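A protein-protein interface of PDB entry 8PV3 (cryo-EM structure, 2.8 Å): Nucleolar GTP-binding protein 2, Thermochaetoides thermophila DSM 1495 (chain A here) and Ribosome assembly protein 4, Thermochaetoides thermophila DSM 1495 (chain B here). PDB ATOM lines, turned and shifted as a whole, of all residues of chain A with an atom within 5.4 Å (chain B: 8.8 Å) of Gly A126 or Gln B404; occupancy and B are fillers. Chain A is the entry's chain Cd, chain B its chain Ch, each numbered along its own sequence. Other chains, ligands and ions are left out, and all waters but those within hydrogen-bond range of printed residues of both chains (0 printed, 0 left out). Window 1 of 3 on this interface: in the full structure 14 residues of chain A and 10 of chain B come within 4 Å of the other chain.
O of Pro A121 is in hydrogen-bond range of NE2 of Gln B404.
O of Lys A122 is in hydrogen-bond range of NE2 of Gln B404.
A ring nitrogen (NE2) of His A130 sits at hydrogen-bond distance from the side-chain amino group of Lys A129, at 3.0 Å.
The side-chain carboxylate (OD1) of Asp B381 sits at hydrogen-bond distance from the side-chain hydroxyl (OG1) of Thr B383 (2.5 Å).
The side-chain carboxylate (OD2) of Asp B425 is in hydrogen-bond range of the backbone NH (N) of Gln B404 (2.8 Å).
Leu A123 touches Gln B404.
O of Gly A126 touches CE2 of Phe B382, at 3.5 Å.
Gln B404 touches Gly A126.
Leu A127 touches Asp B381.
Phe B382 touches Leu A127 (CD2 to CD1, 3.8 Å).
His A130 touches Phe B382.
Gly A126 touches just these residues of chain B: Phe B382 and Gln B404.
Of the printed residues of chain B, His A130 touches Phe B382.
Printed residues of chain A within 4 Å of Phe B382: Gly A126 (3.5 Å), Leu A127 (3.8 Å) and His A130 (3.4 Å).
Of chain A, only Pro A121, Lys A122, Leu A123 and Gly A126 come within 4 Å of Gln B404.
Lys B429 touches none of the printed residues of chain A.
Among the printed residues, no Asp or Glu carboxylate lies within 4 Å of a Lys or Arg side-chain nitrogen of the other chain.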
ATOM      1  N   PRO A 121      -0.414  10.348  -8.881  1.00  0.00           N
ATOM      2  CA  PRO A 121      -1.019   9.629 -10.006  1.00  0.00           C
ATOM      3  C   PRO A 121       0.035   8.918 -10.841  1.00  0.00           C
ATOM      4  O   PRO A 121       1.235   9.180 -10.738  1.00  0.00           O
ATOM      5  CB  PRO A 121      -1.711  10.737 -10.806  1.00  0.00           C
ATOM      6  CG  PRO A 121      -0.931  11.963 -10.482  1.00  0.00           C
ATOM      7  CD  PRO A 121      -0.509  11.809  -9.048  1.00  0.00           C
ATOM      8  N   LYS A 122      -0.440   7.989 -11.667  1.00  0.00           N
ATOM      9  CA  LYS A 122       0.454   7.195 -12.496  1.00  0.00           C
ATOM     10  C   LYS A 122       1.102   8.060 -13.570  1.00  0.00           C
ATOM     11  O   LYS A 122       0.570   9.101 -13.967  1.00  0.00           O
ATOM     12  CB  LYS A 122      -0.309   6.033 -13.137  1.00  0.00           C
ATOM     13  CG  LYS A 122      -0.967   5.021 -12.174  1.00  0.00           C
ATOM     14  CD  LYS A 122       0.016   4.110 -11.412  1.00  0.00           C
ATOM     15  CE  LYS A 122       0.406   4.634 -10.028  1.00  0.00           C
ATOM     16  NZ  LYS A 122       1.271   3.674  -9.284  1.00  0.00           N
ATOM     17  N   LEU A 123       2.280   7.621 -14.028  1.00  0.00           N
ATOM     18  CA  LEU A 123       3.059   8.413 -14.979  1.00  0.00           C
ATOM     19  C   LEU A 123       2.358   8.519 -16.328  1.00  0.00           C
ATOM     20  O   LEU A 123       2.397   9.576 -16.974  1.00  0.00           O
ATOM     21  CB  LEU A 123       4.469   7.821 -15.110  1.00  0.00           C
ATOM     22  CG  LEU A 123       4.764   6.397 -15.612  1.00  0.00           C
ATOM     23  CD1 LEU A 123       4.809   6.258 -17.137  1.00  0.00           C
ATOM     24  CD2 LEU A 123       6.054   5.876 -14.987  1.00  0.00           C
ATOM     25  N   GLU A 124       1.699   7.441 -16.764  1.00  0.00           N
ATOM     26  CA  GLU A 124       0.966   7.475 -18.025  1.00  0.00           C
ATOM     27  C   GLU A 124      -0.210   8.443 -17.949  1.00  0.00           C
ATOM     28  O   GLU A 124      -0.482   9.181 -18.902  1.00  0.00           O
ATOM     29  CB  GLU A 124       0.515   6.060 -18.414  1.00  0.00           C
ATOM     30  CG  GLU A 124      -0.440   5.359 -17.448  1.00  0.00           C
ATOM     31  CD  GLU A 124       0.280   4.575 -16.367  1.00  0.00           C
ATOM     32  OE1 GLU A 124       1.503   4.767 -16.199  1.00  0.00           O
ATOM     33  OE2 GLU A 124      -0.380   3.767 -15.681  1.00  0.00           O
ATOM     34  N   ASP A 125      -0.891   8.488 -16.799  1.00  0.00           N
ATOM     35  CA  ASP A 125      -1.987   9.433 -16.621  1.00  0.00           C
ATOM     36  C   ASP A 125      -1.473  10.865 -16.563  1.00  0.00           C
ATOM     37  O   ASP A 125      -2.090  11.776 -17.126  1.00  0.00           O
ATOM     38  CB  ASP A 125      -2.773   9.094 -15.356  1.00  0.00           C
ATOM     39  CG  ASP A 125      -3.543   7.796 -15.480  1.00  0.00           C
ATOM     40  OD1 ASP A 125      -3.939   7.443 -16.610  1.00  0.00           O
ATOM     41  OD2 ASP A 125      -3.757   7.129 -14.445  1.00  0.00           O
ATOM     42  N   GLY A 126      -0.334  11.077 -15.896  1.00  0.00           N
ATOM     43  CA  GLY A 126       0.231  12.414 -15.811  1.00  0.00           C
ATOM     44  C   GLY A 126       0.700  12.943 -17.153  1.00  0.00           C
ATOM     45  O   GLY A 126       0.616  14.144 -17.420  1.00  0.00           O
ATOM     46  N   LEU A 127       1.211  12.059 -18.009  1.00  0.00           N
ATOM     47  CA  LEU A 127       1.586  12.478 -19.354  1.00  0.00           C
ATOM     48  C   LEU A 127       0.360  12.692 -20.239  1.00  0.00           C
ATOM     49  O   LEU A 127       0.300  13.671 -20.998  1.00  0.00           O
ATOM     50  CB  LEU A 127       2.527  11.446 -19.977  1.00  0.00           C
ATOM     51  CG  LEU A 127       3.570  11.959 -20.971  1.00  0.00           C
ATOM     52  CD1 LEU A 127       4.249  13.214 -20.448  1.00  0.00           C
ATOM     53  CD2 LEU A 127       4.596  10.879 -21.271  1.00  0.00           C
ATOM     54  N   LYS A 128      -0.629  11.797 -20.144  1.00  0.00           N
ATOM     55  CA  LYS A 128      -1.804  11.873 -21.005  1.00  0.00           C
ATOM     56  C   LYS A 128      -2.663  13.088 -20.679  1.00  0.00           C
ATOM     57  O   LYS A 128      -3.248  13.700 -21.582  1.00  0.00           O
ATOM     58  CB  LYS A 128      -2.617  10.583 -20.875  1.00  0.00           C
ATOM     59  CG  LYS A 128      -3.901  10.544 -21.687  1.00  0.00           C
ATOM     60  CD  LYS A 128      -4.634   9.227 -21.494  1.00  0.00           C
ATOM     61  CE  LYS A 128      -5.869   9.146 -22.375  1.00  0.00           C
ATOM     62  NZ  LYS A 128      -6.580   7.850 -22.211  1.00  0.00           N
ATOM     63  N   LYS A 129      -2.741  13.464 -19.400  1.00  0.00           N
ATOM     64  CA  LYS A 129      -3.596  14.574 -19.000  1.00  0.00           C
ATOM     65  C   LYS A 129      -3.068  15.914 -19.502  1.00  0.00           C
ATOM     66  O   LYS A 129      -3.857  16.844 -19.707  1.00  0.00           O
ATOM     67  CB  LYS A 129      -3.748  14.559 -17.473  1.00  0.00           C
ATOM     68  CG  LYS A 129      -4.650  15.630 -16.875  1.00  0.00           C
ATOM     69  CD  LYS A 129      -4.836  15.416 -15.379  1.00  0.00           C
ATOM     70  CE  LYS A 129      -3.578  15.743 -14.596  1.00  0.00           C
ATOM     71  NZ  LYS A 129      -3.283  17.200 -14.624  1.00  0.00           N
ATOM     72  N   HIS A 130      -1.763  16.023 -19.754  1.00  0.00           N
ATOM     73  CA  HIS A 130      -1.181  17.246 -20.288  1.00  0.00           C
ATOM     74  C   HIS A 130      -0.765  17.145 -21.747  1.00  0.00           C
ATOM     75  O   HIS A 130      -0.268  18.138 -22.290  1.00  0.00           O
ATOM     76  CB  HIS A 130       0.038  17.667 -19.459  1.00  0.00           C
ATOM     77  CG  HIS A 130      -0.280  18.005 -18.038  1.00  0.00           C
ATOM     78  ND1 HIS A 130      -0.622  19.277 -17.636  1.00  0.00           N
ATOM     79  CD2 HIS A 130      -0.308  17.238 -16.923  1.00  0.00           C
ATOM     80  CE1 HIS A 130      -0.843  19.281 -16.335  1.00  0.00           C
ATOM     81  NE2 HIS A 130      -0.658  18.056 -15.877  1.00  0.00           N
ATOM     82  N   ASP B 380      10.447  20.445 -20.913  1.00  0.00           N
ATOM     83  CA  ASP B 380       9.093  20.789 -20.482  1.00  0.00           C
ATOM     84  C   ASP B 380       8.086  19.783 -20.874  1.00  0.00           C
ATOM     85  O   ASP B 380       6.946  19.903 -20.416  1.00  0.00           O
ATOM     86  CB  ASP B 380       8.672  22.146 -21.043  1.00  0.00           C
ATOM     87  CG  ASP B 380       9.331  23.293 -20.340  1.00  0.00           C
ATOM     88  OD1 ASP B 380       8.715  24.375 -20.256  1.00  0.00           O
ATOM     89  OD2 ASP B 380      10.459  23.107 -19.853  1.00  0.00           O
ATOM     90  N   ASP B 381       8.414  18.791 -21.697  1.00  0.00           N
ATOM     91  CA  ASP B 381       7.465  17.748 -22.052  1.00  0.00           C
ATOM     92  C   ASP B 381       7.387  16.646 -21.006  1.00  0.00           C
ATOM     93  O   ASP B 381       6.972  15.530 -21.335  1.00  0.00           O
ATOM     94  CB  ASP B 381       7.795  17.161 -23.430  1.00  0.00           C
ATOM     95  CG  ASP B 381       9.202  16.596 -23.526  1.00  0.00           C
ATOM     96  OD1 ASP B 381       9.917  16.509 -22.509  1.00  0.00           O
ATOM     97  OD2 ASP B 381       9.600  16.214 -24.644  1.00  0.00           O
ATOM     98  N   PHE B 382       7.825  16.940 -19.777  1.00  0.00           N
ATOM     99  CA  PHE B 382       7.815  16.083 -18.590  1.00  0.00           C
ATOM    100  C   PHE B 382       8.851  14.975 -18.688  1.00  0.00           C
ATOM    101  O   PHE B 382       8.901  14.102 -17.817  1.00  0.00           O
ATOM    102  CB  PHE B 382       6.447  15.442 -18.284  1.00  0.00           C
ATOM    103  CG  PHE B 382       5.310  16.418 -18.054  1.00  0.00           C
ATOM    104  CD1 PHE B 382       5.499  17.791 -18.006  1.00  0.00           C
ATOM    105  CD2 PHE B 382       4.033  15.929 -17.862  1.00  0.00           C
ATOM    106  CE1 PHE B 382       4.442  18.645 -17.795  1.00  0.00           C
ATOM    107  CE2 PHE B 382       2.979  16.780 -17.643  1.00  0.00           C
ATOM    108  CZ  PHE B 382       3.182  18.140 -17.611  1.00  0.00           C
ATOM    109  N   THR B 383       9.687  14.982 -19.724  1.00  0.00           N
ATOM    110  CA  THR B 383      10.557  13.855 -20.005  1.00  0.00           C
ATOM    111  C   THR B 383      12.007  14.306 -20.033  1.00  0.00           C
ATOM    112  O   THR B 383      12.334  15.505 -19.979  1.00  0.00           O
ATOM    113  CB  THR B 383      10.229  13.177 -21.341  1.00  0.00           C
ATOM    114  OG1 THR B 383      10.510  14.080 -22.415  1.00  0.00           O
ATOM    115  CG2 THR B 383       8.766  12.792 -21.401  1.00  0.00           C
ATOM    116  N   LEU B 401      11.546   8.708 -17.843  1.00  0.00           N
ATOM    117  CA  LEU B 401      10.110   8.928 -17.741  1.00  0.00           C
ATOM    118  C   LEU B 401       9.664   8.759 -16.297  1.00  0.00           C
ATOM    119  O   LEU B 401      10.084   7.832 -15.601  1.00  0.00           O
ATOM    120  CB  LEU B 401       9.329   7.935 -18.612  1.00  0.00           C
ATOM    121  CG  LEU B 401       9.313   8.073 -20.129  1.00  0.00           C
ATOM    122  CD1 LEU B 401       8.709   6.832 -20.747  1.00  0.00           C
ATOM    123  CD2 LEU B 401       8.501   9.276 -20.508  1.00  0.00           C
ATOM    124  N   GLY B 402       8.761   9.635 -15.865  1.00  0.00           N
ATOM    125  CA  GLY B 402       8.179   9.542 -14.544  1.00  0.00           C
ATOM    126  C   GLY B 402       7.890  10.863 -13.867  1.00  0.00           C
ATOM    127  O   GLY B 402       7.144  10.878 -12.883  1.00  0.00           O
ATOM    128  N   HIS B 403       8.446  11.964 -14.358  1.00  0.00           N
ATOM    129  CA  HIS B 403       8.129  13.264 -13.787  1.00  0.00           C
ATOM    130  C   HIS B 403       6.744  13.705 -14.240  1.00  0.00           C
ATOM    131  O   HIS B 403       6.413  13.646 -15.427  1.00  0.00           O
ATOM    132  CB  HIS B 403       9.177  14.295 -14.198  1.00  0.00           C
ATOM    133  CG  HIS B 403      10.273  14.476 -13.195  1.00  0.00           C
ATOM    134  ND1 HIS B 403      10.074  15.084 -11.975  1.00  0.00           N
ATOM    135  CD2 HIS B 403      11.581  14.127 -13.232  1.00  0.00           C
ATOM    136  CE1 HIS B 403      11.212  15.102 -11.304  1.00  0.00           C
ATOM    137  NE2 HIS B 403      12.141  14.527 -12.044  1.00  0.00           N
ATOM    138  N   GLN B 404       5.927  14.140 -13.286  1.00  0.00           N
ATOM    139  CA  GLN B 404       4.563  14.565 -13.568  1.00  0.00           C
ATOM    140  C   GLN B 404       4.462  16.028 -13.963  1.00  0.00           C
ATOM    141  O   GLN B 404       3.360  16.496 -14.266  1.00  0.00           O
ATOM    142  CB  GLN B 404       3.665  14.300 -12.358  1.00  0.00           C
ATOM    143  CG  GLN B 404       3.639  12.854 -11.919  1.00  0.00           C
ATOM    144  CD  GLN B 404       2.925  11.970 -12.915  1.00  0.00           C
ATOM    145  OE1 GLN B 404       3.523  11.482 -13.871  1.00  0.00           O
ATOM    146  NE2 GLN B 404       1.632  11.769 -12.703  1.00  0.00           N
ATOM    147  N   ASN B 405       5.570  16.758 -13.961  1.00  0.00           N
ATOM    148  CA  ASN B 405       5.580  18.141 -14.403  1.00  0.00           C
ATOM    149  C   ASN B 405       6.926  18.404 -15.064  1.00  0.00           C
ATOM    150  O   ASN B 405       7.722  17.486 -15.274  1.00  0.00           O
ATOM    151  CB  ASN B 405       5.294  19.092 -13.239  1.00  0.00           C
ATOM    152  CG  ASN B 405       4.619  20.370 -13.684  1.00  0.00           C
ATOM    153  OD1 ASN B 405       4.603  20.696 -14.867  1.00  0.00           O
ATOM    154  ND2 ASN B 405       4.041  21.095 -12.735  1.00  0.00           N
ATOM    155  N   LYS B 406       7.162  19.666 -15.419  1.00  0.00           N
ATOM    156  CA  LYS B 406       8.365  20.045 -16.147  1.00  0.00           C
ATOM    157  C   LYS B 406       9.611  19.808 -15.306  1.00  0.00           C
ATOM    158  O   LYS B 406       9.608  20.015 -14.092  1.00  0.00           O
ATOM    159  CB  LYS B 406       8.282  21.515 -16.556  1.00  0.00           C
ATOM    160  CG  LYS B 406       6.992  21.885 -17.255  1.00  0.00           C
ATOM    161  CD  LYS B 406       6.948  23.363 -17.595  1.00  0.00           C
ATOM    162  CE  LYS B 406       6.921  24.216 -16.344  1.00  0.00           C
ATOM    163  NZ  LYS B 406       5.686  23.981 -15.557  1.00  0.00           N
ATOM    164  N   VAL B 407      10.676  19.355 -15.959  1.00  0.00           N
ATOM    165  CA  VAL B 407      11.952  19.105 -15.302  1.00  0.00           C
ATOM    166  C   VAL B 407      12.828  20.333 -15.498  1.00  0.00           C
ATOM    167  O   VAL B 407      13.143  20.708 -16.633  1.00  0.00           O
ATOM    168  CB  VAL B 407      12.634  17.843 -15.849  1.00  0.00           C
ATOM    169  CG1 VAL B 407      13.773  17.434 -14.940  1.00  0.00           C
ATOM    170  CG2 VAL B 407      11.631  16.715 -15.984  1.00  0.00           C
ATOM    171  N   GLY B 423      12.088  18.484 -10.559  1.00  0.00           N
ATOM    172  CA  GLY B 423      10.926  18.763 -11.367  1.00  0.00           C
ATOM    173  C   GLY B 423      10.023  19.794 -10.718  1.00  0.00           C
ATOM    174  O   GLY B 423      10.190  20.161  -9.553  1.00  0.00           O
ATOM    175  N   TRP B 424       9.054  20.257 -11.504  1.00  0.00           N
ATOM    176  CA  TRP B 424       8.022  21.166 -11.028  1.00  0.00           C
ATOM    177  C   TRP B 424       6.882  20.435 -10.333  1.00  0.00           C
ATOM    178  O   TRP B 424       5.944  21.082  -9.856  1.00  0.00           O
ATOM    179  CB  TRP B 424       7.476  22.001 -12.190  1.00  0.00           C
ATOM    180  CG  TRP B 424       8.410  23.071 -12.679  1.00  0.00           C
ATOM    181  CD1 TRP B 424       9.704  22.915 -13.078  1.00  0.00           C
ATOM    182  CD2 TRP B 424       8.106  24.459 -12.846  1.00  0.00           C
ATOM    183  NE1 TRP B 424      10.228  24.119 -13.471  1.00  0.00           N
ATOM    184  CE2 TRP B 424       9.267  25.084 -13.338  1.00  0.00           C
ATOM    185  CE3 TRP B 424       6.968  25.236 -12.620  1.00  0.00           C
ATOM    186  CZ2 TRP B 424       9.323  26.447 -13.608  1.00  0.00           C
ATOM    187  CZ3 TRP B 424       7.025  26.588 -12.889  1.00  0.00           C
ATOM    188  CH2 TRP B 424       8.194  27.180 -13.377  1.00  0.00           C
ATOM    189  N   ASP B 425       6.945  19.105 -10.264  1.00  0.00           N
ATOM    190  CA  ASP B 425       5.984  18.297  -9.528  1.00  0.00           C
ATOM    191  C   ASP B 425       6.413  18.076  -8.085  1.00  0.00           C
ATOM    192  O   ASP B 425       6.092  17.034  -7.504  1.00  0.00           O
ATOM    193  CB  ASP B 425       5.778  16.950 -10.220  1.00  0.00           C
ATOM    194  CG  ASP B 425       7.081  16.251 -10.528  1.00  0.00           C
ATOM    195  OD1 ASP B 425       8.144  16.894 -10.420  1.00  0.00           O
ATOM    196  OD2 ASP B 425       7.048  15.052 -10.866  1.00  0.00           O
ATOM    197  N   ASN B 426       7.174  19.021  -7.526  1.00  0.00           N
ATOM    198  CA  ASN B 426       7.643  19.052  -6.145  1.00  0.00           C
ATOM    199  C   ASN B 426       8.593  17.905  -5.821  1.00  0.00           C
ATOM    200  O   ASN B 426       8.779  17.575  -4.648  1.00  0.00           O
ATOM    201  CB  ASN B 426       6.477  19.037  -5.146  1.00  0.00           C
ATOM    202  CG  ASN B 426       5.429  20.082  -5.453  1.00  0.00           C
ATOM    203  OD1 ASN B 426       5.736  21.163  -5.936  1.00  0.00           O
ATOM    204  ND2 ASN B 426       4.177  19.760  -5.162  1.00  0.00           N
ATOM    205  N   SER B 427       9.211  17.286  -6.824  1.00  0.00           N
ATOM    206  CA  SER B 427       9.924  16.038  -6.611  1.00  0.00           C
ATOM    207  C   SER B 427      11.305  16.058  -7.254  1.00  0.00           C
ATOM    208  O   SER B 427      11.537  16.687  -8.292  1.00  0.00           O
ATOM    209  CB  SER B 427       9.128  14.846  -7.151  1.00  0.00           C
ATOM    210  OG  SER B 427       9.189  14.796  -8.565  1.00  0.00           O
ATOM    211  N   LYS B 429      14.131  13.173  -8.539  1.00  0.00           N
ATOM    212  CA  LYS B 429      14.189  11.771  -8.923  1.00  0.00           C
ATOM    213  C   LYS B 429      15.610  11.363  -9.284  1.00  0.00           C
ATOM    214  O   LYS B 429      16.379  12.155  -9.842  1.00  0.00           O
ATOM    215  CB  LYS B 429      13.242  11.480 -10.086  1.00  0.00           C
ATOM    216  CG  LYS B 429      11.785  11.483  -9.672  1.00  0.00           C
ATOM    217  CD  LYS B 429      10.873  11.061 -10.799  1.00  0.00           C
ATOM    218  CE  LYS B 429       9.474  10.788 -10.284  1.00  0.00           C
ATOM    219  NZ  LYS B 429       8.875  11.992  -9.656  1.00  0.00           N
ATOM    220  N   TRP B 431      18.253   8.437 -11.055  1.00  0.00           N
ATOM    221  CA  TRP B 431      18.256   7.659 -12.278  1.00  0.00           C
ATOM    222  C   TRP B 431      19.600   6.959 -12.387  1.00  0.00           C
ATOM    223  O   TRP B 431      20.632   7.528 -12.028  1.00  0.00           O
ATOM    224  CB  TRP B 431      18.064   8.579 -13.480  1.00  0.00           C
ATOM    225  CG  TRP B 431      16.796   9.363 -13.425  1.00  0.00           C
ATOM    226  CD1 TRP B 431      16.643  10.613 -12.903  1.00  0.00           C
ATOM    227  CD2 TRP B 431      15.514   8.981 -13.926  1.00  0.00           C
ATOM    228  NE1 TRP B 431      15.346  11.027 -13.032  1.00  0.00           N
ATOM    229  CE2 TRP B 431      14.631  10.045 -13.663  1.00  0.00           C
ATOM    230  CE3 TRP B 431      15.026   7.845 -14.576  1.00  0.00           C
ATOM    231  CZ2 TRP B 431      13.292  10.005 -14.016  1.00  0.00           C
ATOM    232  CZ3 TRP B 431      13.697   7.810 -14.924  1.00  0.00           C
ATOM    233  CH2 TRP B 431      12.845   8.881 -14.643  1.00  0.00           C
ATOM    234  N   ASN B 441      12.417   8.053  -5.655  1.00  0.00           N
ATOM    235  CA  ASN B 441      11.831   9.383  -5.657  1.00  0.00           C
ATOM    236  C   ASN B 441      12.012  10.025  -4.289  1.00  0.00           C
ATOM    237  O   ASN B 441      11.735   9.403  -3.260  1.00  0.00           O
ATOM    238  CB  ASN B 441      10.346   9.320  -6.012  1.00  0.00           C
ATOM    239  CG  ASN B 441       9.722  10.689  -6.153  1.00  0.00           C
ATOM    240  OD1 ASN B 441      10.386  11.649  -6.538  1.00  0.00           O
ATOM    241  ND2 ASN B 441       8.437  10.787  -5.840  1.00  0.00           N
